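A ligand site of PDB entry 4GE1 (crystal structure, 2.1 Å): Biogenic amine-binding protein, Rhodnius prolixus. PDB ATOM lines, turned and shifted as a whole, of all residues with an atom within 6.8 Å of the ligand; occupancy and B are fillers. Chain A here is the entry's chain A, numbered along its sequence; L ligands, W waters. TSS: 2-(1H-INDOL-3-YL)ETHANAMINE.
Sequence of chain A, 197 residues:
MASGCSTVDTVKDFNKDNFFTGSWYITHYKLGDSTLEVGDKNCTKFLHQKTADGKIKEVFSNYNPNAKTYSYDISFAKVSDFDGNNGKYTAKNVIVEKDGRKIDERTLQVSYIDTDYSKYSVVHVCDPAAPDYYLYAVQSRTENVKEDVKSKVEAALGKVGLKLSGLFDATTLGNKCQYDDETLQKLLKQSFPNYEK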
ATOM      1  N   ILE A  26      13.153  14.220 -20.838  1.00  0.00           N
ATOM      2  CA  ILE A  26      12.807  13.255 -19.797  1.00  0.00           C
ATOM      3  C   ILE A  26      12.542  11.898 -20.455  1.00  0.00           C
ATOM      4  O   ILE A  26      11.533  11.715 -21.134  1.00  0.00           O
ATOM      5  CB  ILE A  26      11.600  13.715 -18.971  1.00  0.00           C
ATOM      6  CG1 ILE A  26      11.863  15.126 -18.438  1.00  0.00           C
ATOM      7  CG2 ILE A  26      11.338  12.741 -17.826  1.00  0.00           C
ATOM      8  CD1 ILE A  26      10.941  15.552 -17.327  1.00  0.00           C
ATOM      9  N   THR A  44       8.397  14.836 -22.438  1.00  0.00           N
ATOM     10  CA  THR A  44       8.724  16.140 -21.882  1.00  0.00           C
ATOM     11  C   THR A  44      10.109  16.611 -22.306  1.00  0.00           C
ATOM     12  O   THR A  44      11.086  15.865 -22.238  1.00  0.00           O
ATOM     13  CB  THR A  44       8.590  16.171 -20.348  1.00  0.00           C
ATOM     14  OG1 THR A  44       7.206  16.060 -19.963  1.00  0.00           O
ATOM     15  CG2 THR A  44       9.154  17.499 -19.812  1.00  0.00           C
ATOM     16  N   PHE A  46      12.516  20.184 -21.645  1.00  0.00           N
ATOM     17  CA  PHE A  46      12.547  21.481 -21.003  1.00  0.00           C
ATOM     18  C   PHE A  46      13.784  22.312 -21.324  1.00  0.00           C
ATOM     19  O   PHE A  46      14.836  21.781 -21.677  1.00  0.00           O
ATOM     20  CB  PHE A  46      12.207  21.451 -19.496  1.00  0.00           C
ATOM     21  CG  PHE A  46      13.149  20.634 -18.634  1.00  0.00           C
ATOM     22  CD1 PHE A  46      14.065  21.276 -17.804  1.00  0.00           C
ATOM     23  CD2 PHE A  46      13.069  19.250 -18.591  1.00  0.00           C
ATOM     24  CE1 PHE A  46      14.919  20.550 -16.967  1.00  0.00           C
ATOM     25  CE2 PHE A  46      13.913  18.512 -17.741  1.00  0.00           C
ATOM     26  CZ  PHE A  46      14.843  19.163 -16.941  1.00  0.00           C
ATOM     27  N   GLU A  58      12.984  27.689 -15.758  1.00  0.00           N
ATOM     28  CA  GLU A  58      12.918  26.397 -16.439  1.00  0.00           C
ATOM     29  C   GLU A  58      11.540  26.190 -17.056  1.00  0.00           C
ATOM     30  O   GLU A  58      10.535  26.190 -16.344  1.00  0.00           O
ATOM     31  CB  GLU A  58      13.232  25.254 -15.472  1.00  0.00           C
ATOM     32  CG  GLU A  58      14.412  25.520 -14.542  1.00  0.00           C
ATOM     33  CD  GLU A  58      14.744  24.324 -13.663  1.00  0.00           C
ATOM     34  OE1 GLU A  58      15.249  23.311 -14.200  1.00  0.00           O
ATOM     35  OE2 GLU A  58      14.507  24.402 -12.437  1.00  0.00           O
ATOM     36  N   PHE A  60       8.878  23.975 -19.314  1.00  0.00           N
ATOM     37  CA  PHE A  60       8.582  22.592 -19.698  1.00  0.00           C
ATOM     38  C   PHE A  60       7.505  22.505 -20.771  1.00  0.00           C
ATOM     39  O   PHE A  60       6.476  23.171 -20.685  1.00  0.00           O
ATOM     40  CB  PHE A  60       8.144  21.774 -18.483  1.00  0.00           C
ATOM     41  CG  PHE A  60       9.190  21.669 -17.385  1.00  0.00           C
ATOM     42  CD1 PHE A  60       9.355  22.692 -16.463  1.00  0.00           C
ATOM     43  CD2 PHE A  60       9.971  20.527 -17.254  1.00  0.00           C
ATOM     44  CE1 PHE A  60      10.296  22.585 -15.448  1.00  0.00           C
ATOM     45  CE2 PHE A  60      10.925  20.415 -16.236  1.00  0.00           C
ATOM     46  CZ  PHE A  60      11.086  21.447 -15.339  1.00  0.00           C
ATOM     47  N   ASN A  62       5.144  19.536 -22.067  1.00  0.00           N
ATOM     48  CA  ASN A  62       4.718  18.156 -21.866  1.00  0.00           C
ATOM     49  C   ASN A  62       3.685  17.755 -22.900  1.00  0.00           C
ATOM     50  O   ASN A  62       2.592  18.315 -22.922  1.00  0.00           O
ATOM     51  CB  ASN A  62       4.128  17.965 -20.474  1.00  0.00           C
ATOM     52  CG  ASN A  62       4.959  18.614 -19.412  1.00  0.00           C
ATOM     53  OD1 ASN A  62       6.090  18.219 -19.160  1.00  0.00           O
ATOM     54  ND2 ASN A  62       4.394  19.625 -18.761  1.00  0.00           N
ATOM     55  N   ASP A  73       4.568  24.182 -18.092  1.00  0.00           N
ATOM     56  CA  ASP A  73       4.811  24.709 -16.751  1.00  0.00           C
ATOM     57  C   ASP A  73       6.198  25.351 -16.660  1.00  0.00           C
ATOM     58  O   ASP A  73       7.062  25.111 -17.513  1.00  0.00           O
ATOM     59  CB  ASP A  73       4.594  23.651 -15.640  1.00  0.00           C
ATOM     60  CG  ASP A  73       5.455  22.418 -15.798  1.00  0.00           C
ATOM     61  OD1 ASP A  73       4.999  21.456 -16.448  1.00  0.00           O
ATOM     62  OD2 ASP A  73       6.578  22.391 -15.228  1.00  0.00           O
ATOM     63  N   ILE A  74       6.383  26.200 -15.670  1.00  0.00           N
ATOM     64  CA  ILE A  74       7.637  26.928 -15.546  1.00  0.00           C
ATOM     65  C   ILE A  74       8.095  26.966 -14.112  1.00  0.00           C
ATOM     66  O   ILE A  74       7.321  27.306 -13.216  1.00  0.00           O
ATOM     67  CB  ILE A  74       7.491  28.380 -16.037  1.00  0.00           C
ATOM     68  CG1 ILE A  74       6.849  28.427 -17.431  1.00  0.00           C
ATOM     69  CG2 ILE A  74       8.848  29.085 -16.018  1.00  0.00           C
ATOM     70  CD1 ILE A  74       6.468  29.827 -17.897  1.00  0.00           C
ATOM     71  N   SER A  75       9.360  26.606 -13.898  1.00  0.00           N
ATOM     72  CA  SER A  75       9.952  26.725 -12.570  1.00  0.00           C
ATOM     73  C   SER A  75      10.762  28.001 -12.463  1.00  0.00           C
ATOM     74  O   SER A  75      11.590  28.307 -13.326  1.00  0.00           O
ATOM     75  CB  SER A  75      10.837  25.525 -12.255  1.00  0.00           C
ATOM     76  OG  SER A  75      10.076  24.352 -12.155  1.00  0.00           O
ATOM     77  N   TYR A  89      17.319  22.270  -4.359  1.00  0.00           N
ATOM     78  CA  TYR A  89      16.724  23.589  -4.279  1.00  0.00           C
ATOM     79  C   TYR A  89      15.208  23.513  -4.254  1.00  0.00           C
ATOM     80  O   TYR A  89      14.618  22.474  -4.533  1.00  0.00           O
ATOM     81  CB  TYR A  89      17.191  24.494  -5.432  1.00  0.00           C
ATOM     82  CG  TYR A  89      16.809  24.034  -6.829  1.00  0.00           C
ATOM     83  CD1 TYR A  89      15.800  24.683  -7.541  1.00  0.00           C
ATOM     84  CD2 TYR A  89      17.452  22.971  -7.440  1.00  0.00           C
ATOM     85  CE1 TYR A  89      15.438  24.268  -8.828  1.00  0.00           C
ATOM     86  CE2 TYR A  89      17.102  22.551  -8.723  1.00  0.00           C
ATOM     87  CZ  TYR A  89      16.096  23.204  -9.412  1.00  0.00           C
ATOM     88  OH  TYR A  89      15.754  22.796 -10.678  1.00  0.00           O
ATOM     89  N   ALA A  91      11.709  25.461  -5.779  1.00  0.00           N
ATOM     90  CA  ALA A  91      11.267  26.321  -6.859  1.00  0.00           C
ATOM     91  C   ALA A  91       9.772  26.547  -6.737  1.00  0.00           C
ATOM     92  O   ALA A  91       9.047  25.723  -6.173  1.00  0.00           O
ATOM     93  CB  ALA A  91      11.620  25.697  -8.207  1.00  0.00           C
ATOM     94  N   ASN A  93       6.716  26.488  -9.013  1.00  0.00           N
ATOM     95  CA  ASN A  93       6.386  25.996 -10.338  1.00  0.00           C
ATOM     96  C   ASN A  93       4.965  26.387 -10.707  1.00  0.00           C
ATOM     97  O   ASN A  93       4.028  26.186  -9.936  1.00  0.00           O
ATOM     98  CB  ASN A  93       6.609  24.482 -10.450  1.00  0.00           C
ATOM     99  CG  ASN A  93       6.255  23.933 -11.836  1.00  0.00           C
ATOM    100  OD1 ASN A  93       5.108  23.562 -12.083  1.00  0.00           O
ATOM    101  ND2 ASN A  93       7.231  23.872 -12.729  1.00  0.00           N
ATOM    102  N   ILE A  95       1.900  26.230 -13.495  1.00  0.00           N
ATOM    103  CA  ILE A  95       1.290  25.584 -14.642  1.00  0.00           C
ATOM    104  C   ILE A  95       0.659  26.694 -15.468  1.00  0.00           C
ATOM    105  O   ILE A  95      -0.143  27.464 -14.937  1.00  0.00           O
ATOM    106  CB  ILE A  95       0.194  24.578 -14.227  1.00  0.00           C
ATOM    107  CG1 ILE A  95       0.711  23.624 -13.137  1.00  0.00           C
ATOM    108  CG2 ILE A  95      -0.349  23.818 -15.421  1.00  0.00           C
ATOM    109  CD1 ILE A  95       1.902  22.805 -13.561  1.00  0.00           C
ATOM    110  N   ARG A 106       2.539  25.884  -7.553  1.00  0.00           N
ATOM    111  CA  ARG A 106       2.893  25.012  -6.442  1.00  0.00           C
ATOM    112  C   ARG A 106       4.372  25.172  -6.118  1.00  0.00           C
ATOM    113  O   ARG A 106       5.145  25.744  -6.900  1.00  0.00           O
ATOM    114  CB  ARG A 106       2.659  23.569  -6.854  1.00  0.00           C
ATOM    115  CG  ARG A 106       3.518  23.177  -8.028  1.00  0.00           C
ATOM    116  CD  ARG A 106       2.975  21.981  -8.772  1.00  0.00           C
ATOM    117  NE  ARG A 106       3.506  21.944 -10.133  1.00  0.00           N
ATOM    118  CZ  ARG A 106       3.560  20.847 -10.880  1.00  0.00           C
ATOM    119  NH1 ARG A 106       3.112  19.689 -10.407  1.00  0.00           N
ATOM    120  NH2 ARG A 106       4.060  20.900 -12.109  1.00  0.00           N
ATOM    121  N   LEU A 108       7.881  23.162  -5.427  1.00  0.00           N
ATOM    122  CA  LEU A 108       8.534  21.884  -5.712  1.00  0.00           C
ATOM    123  C   LEU A 108       9.906  21.813  -5.073  1.00  0.00           C
ATOM    124  O   LEU A 108      10.738  22.711  -5.267  1.00  0.00           O
ATOM    125  CB  LEU A 108       8.666  21.655  -7.221  1.00  0.00           C
ATOM    126  CG  LEU A 108       7.362  21.498  -8.006  1.00  0.00           C
ATOM    127  CD1 LEU A 108       7.606  21.331  -9.496  1.00  0.00           C
ATOM    128  CD2 LEU A 108       6.608  20.312  -7.475  1.00  0.00           C
ATOM    129  N   GLN A 109      10.144  20.764  -4.297  1.00  0.00           N
ATOM    130  CA  GLN A 109      11.483  20.508  -3.774  1.00  0.00           C
ATOM    131  C   GLN A 109      12.232  19.621  -4.756  1.00  0.00           C
ATOM    132  O   GLN A 109      11.807  18.497  -5.043  1.00  0.00           O
ATOM    133  CB  GLN A 109      11.388  19.836  -2.403  1.00  0.00           C
ATOM    134  CG  GLN A 109      10.460  20.572  -1.436  1.00  0.00           C
ATOM    135  CD  GLN A 109      10.389  19.915  -0.064  1.00  0.00           C
ATOM    136  OE1 GLN A 109      10.943  18.839   0.168  1.00  0.00           O
ATOM    137  NE2 GLN A 109       9.704  20.580   0.874  1.00  0.00           N
ATOM    138  N   VAL A 110      13.351  20.127  -5.288  1.00  0.00           N
ATOM    139  CA  VAL A 110      14.095  19.412  -6.310  1.00  0.00           C
ATOM    140  C   VAL A 110      15.397  18.846  -5.742  1.00  0.00           C
ATOM    141  O   VAL A 110      16.150  19.555  -5.069  1.00  0.00           O
ATOM    142  CB  VAL A 110      14.421  20.328  -7.515  1.00  0.00           C
ATOM    143  CG1 VAL A 110      15.030  19.524  -8.652  1.00  0.00           C
ATOM    144  CG2 VAL A 110      13.173  21.076  -7.986  1.00  0.00           C
ATOM    145  N   TYR A 112      18.718  16.726  -7.127  1.00  0.00           N
ATOM    146  CA  TYR A 112      19.507  16.005  -8.121  1.00  0.00           C
ATOM    147  C   TYR A 112      20.387  14.932  -7.470  1.00  0.00           C
ATOM    148  O   TYR A 112      21.315  15.220  -6.714  1.00  0.00           O
ATOM    149  CB  TYR A 112      20.291  16.948  -9.038  1.00  0.00           C
ATOM    150  CG  TYR A 112      19.422  17.471 -10.158  1.00  0.00           C
ATOM    151  CD1 TYR A 112      18.786  18.697 -10.058  1.00  0.00           C
ATOM    152  CD2 TYR A 112      19.195  16.710 -11.301  1.00  0.00           C
ATOM    153  CE1 TYR A 112      17.963  19.166 -11.067  1.00  0.00           C
ATOM    154  CE2 TYR A 112      18.371  17.169 -12.321  1.00  0.00           C
ATOM    155  CZ  TYR A 112      17.755  18.402 -12.199  1.00  0.00           C
ATOM    156  OH  TYR A 112      16.934  18.866 -13.196  1.00  0.00           O
ATOM    157  N   VAL A 123      16.809  12.821 -11.115  1.00  0.00           N
ATOM    158  CA  VAL A 123      16.195  13.797 -10.228  1.00  0.00           C
ATOM    159  C   VAL A 123      15.032  13.225  -9.442  1.00  0.00           C
ATOM    160  O   VAL A 123      14.359  12.300  -9.881  1.00  0.00           O
ATOM    161  CB  VAL A 123      15.763  15.087 -11.009  1.00  0.00           C
ATOM    162  CG1 VAL A 123      14.525  14.812 -11.895  1.00  0.00           C
ATOM    163  CG2 VAL A 123      15.520  16.243 -10.057  1.00  0.00           C
ATOM    164  N   VAL A 125      11.638  14.927  -7.710  1.00  0.00           N
ATOM    165  CA  VAL A 125      10.835  16.140  -7.559  1.00  0.00           C
ATOM    166  C   VAL A 125       9.591  15.851  -6.742  1.00  0.00           C
ATOM    167  O   VAL A 125       8.914  14.845  -6.975  1.00  0.00           O
ATOM    168  CB  VAL A 125      10.406  16.715  -8.900  1.00  0.00           C
ATOM    169  CG1 VAL A 125       9.722  18.061  -8.700  1.00  0.00           C
ATOM    170  CG2 VAL A 125      11.598  16.833  -9.834  1.00  0.00           C
ATOM    171  N   TYR A 133       2.050  13.081  -5.081  1.00  0.00           N
ATOM    172  CA  TYR A 133       2.695  13.402  -6.348  1.00  0.00           C
ATOM    173  C   TYR A 133       4.198  13.515  -6.119  1.00  0.00           C
ATOM    174  O   TYR A 133       4.695  14.570  -5.700  1.00  0.00           O
ATOM    175  CB  TYR A 133       2.172  14.711  -6.936  1.00  0.00           C
ATOM    176  CG  TYR A 133       3.143  15.371  -7.914  1.00  0.00           C
ATOM    177  CD1 TYR A 133       3.199  14.971  -9.250  1.00  0.00           C
ATOM    178  CD2 TYR A 133       3.994  16.392  -7.514  1.00  0.00           C
ATOM    179  CE1 TYR A 133       4.079  15.564 -10.139  1.00  0.00           C
ATOM    180  CE2 TYR A 133       4.881  16.986  -8.395  1.00  0.00           C
ATOM    181  CZ  TYR A 133       4.906  16.567  -9.711  1.00  0.00           C
ATOM    182  OH  TYR A 133       5.780  17.158 -10.607  1.00  0.00           O
ATOM    183  N   LEU A 135       7.999  12.488  -8.131  1.00  0.00           N
ATOM    184  CA  LEU A 135       8.548  12.094  -9.402  1.00  0.00           C
ATOM    185  C   LEU A 135      10.012  11.708  -9.272  1.00  0.00           C
ATOM    186  O   LEU A 135      10.816  12.453  -8.685  1.00  0.00           O
ATOM    187  CB  LEU A 135       8.410  13.239 -10.410  1.00  0.00           C
ATOM    188  CG  LEU A 135       8.965  13.014 -11.814  1.00  0.00           C
ATOM    189  CD1 LEU A 135       8.018  12.122 -12.579  1.00  0.00           C
ATOM    190  CD2 LEU A 135       9.147  14.346 -12.529  1.00  0.00           C
ATOM    191  N   ALA A 137      12.907  10.926 -12.017  1.00  0.00           N
ATOM    192  CA  ALA A 137      13.089  11.075 -13.461  1.00  0.00           C
ATOM    193  C   ALA A 137      14.527  10.910 -13.938  1.00  0.00           C
ATOM    194  O   ALA A 137      15.461  11.433 -13.346  1.00  0.00           O
ATOM    195  CB  ALA A 137      12.540  12.444 -13.928  1.00  0.00           C
ATOM    196  N   GLN A 139      16.888  11.948 -17.071  1.00  0.00           N
ATOM    197  CA  GLN A 139      16.910  13.056 -18.024  1.00  0.00           C
ATOM    198  C   GLN A 139      18.169  13.019 -18.883  1.00  0.00           C
ATOM    199  O   GLN A 139      19.248  12.658 -18.409  1.00  0.00           O
ATOM    200  CB  GLN A 139      16.755  14.383 -17.283  1.00  0.00           C
ATOM    201  CG  GLN A 139      15.550  14.392 -16.329  1.00  0.00           C
ATOM    202  CD  GLN A 139      15.383  15.697 -15.557  1.00  0.00           C
ATOM    203  OE1 GLN A 139      14.268  16.132 -15.301  1.00  0.00           O
ATOM    204  NE2 GLN A 139      16.494  16.315 -15.185  1.00  0.00           N
HETATM  205  N1  TSS L   1       7.931  20.115 -14.796  1.00  0.00           N
HETATM  206  CA  TSS L   1       7.540  19.603 -13.509  1.00  0.00           C
HETATM  207  CB  TSS L   1       8.234  18.371 -13.019  1.00  0.00           C
HETATM  208  CG  TSS L   1       9.694  18.227 -13.326  1.00  0.00           C
HETATM  209  CD1 TSS L   1      10.266  17.322 -14.206  1.00  0.00           C
HETATM  210  NE1 TSS L   1      11.602  17.479 -14.208  1.00  0.00           N
HETATM  211  CE2 TSS L   1      11.935  18.502 -13.332  1.00  0.00           C
HETATM  212  CD2 TSS L   1      10.778  18.973 -12.780  1.00  0.00           C
HETATM  213  CZ2 TSS L   1      13.197  19.067 -12.978  1.00  0.00           C
HETATM  214  CH2 TSS L   1      13.252  20.098 -12.051  1.00  0.00           C
HETATM  215  CZ3 TSS L   1      12.068  20.580 -11.476  1.00  0.00           C
HETATM  216  CE3 TSS L   1      10.835  20.037 -11.835  1.00  0.00           C
HETATM  217  O   HOH W   1       7.194  17.929 -16.614  1.00  0.00           O
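The backbone NH (N) of Phe 60 lies within hydrogen-bond range of the backbone carbonyl oxygen (O) of Asp 73. The side-chain amide nitrogen of Asn 93 is in hydrogen-bond range of the side-chain carboxylate of Asp 73, at 3.0 Å. The side-chain carboxylate of Asp 73 sits at hydrogen-bond distance from the side-chain amide nitrogen of Asn 62 (3.0 Å). The side-chain amide nitrogen (NE2) of Gln 139 lies within hydrogen-bond range of the side-chain hydroxyl (OH) of Tyr 112 (3.3 Å). The backbone NH of Leu 135 lies within hydrogen-bond range of the backbone carbonyl oxygen of Val 125 (2.8 Å). N of Ile 26 lies within hydrogen-bond range of O of Thr 44 (3.0 Å). The side-chain carboxylate of Glu 58 sits at hydrogen-bond distance from the side-chain hydroxyl of Tyr 89, at 2.7 Å. O of Arg 106 lies within hydrogen-bond range of N of Asn 93, 2.7 Å away.
Ile 26 touches the ligand. Phe 60 touches the ligand. OH of Tyr 89 touches CH2 of the ligand, 3.9 Å away. Arg 106 touches the ligand. CG2 of Val 110 touches CZ3 of the ligand, 3.7 Å away. Tyr 112 touches the ligand. Val 125 touches the ligand (CG2 to CD2, 3.7 Å). Tyr 133 touches the ligand. Leu 135 touches the ligand. 11 residues have an atom within 4 Å of the ligand: Ile 26, Phe 60, Asp 73, Tyr 89, Arg 106, Val 110, Tyr 112, Val 125, Tyr 133, Leu 135 and Gln 139. The nearest printed residue that does not touch the ligand is Leu 108 (4.2 Å).
OD2 of Asp 73 is in salt-bridge range of N1 of the ligand (2.7 Å). OE1 of Gln 139 sits at hydrogen-bond distance from NE1 of the ligand (3.2 Å).
Water W1 lies within hydrogen-bond range of OD1 of Asn 62 and N1 of the ligand.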
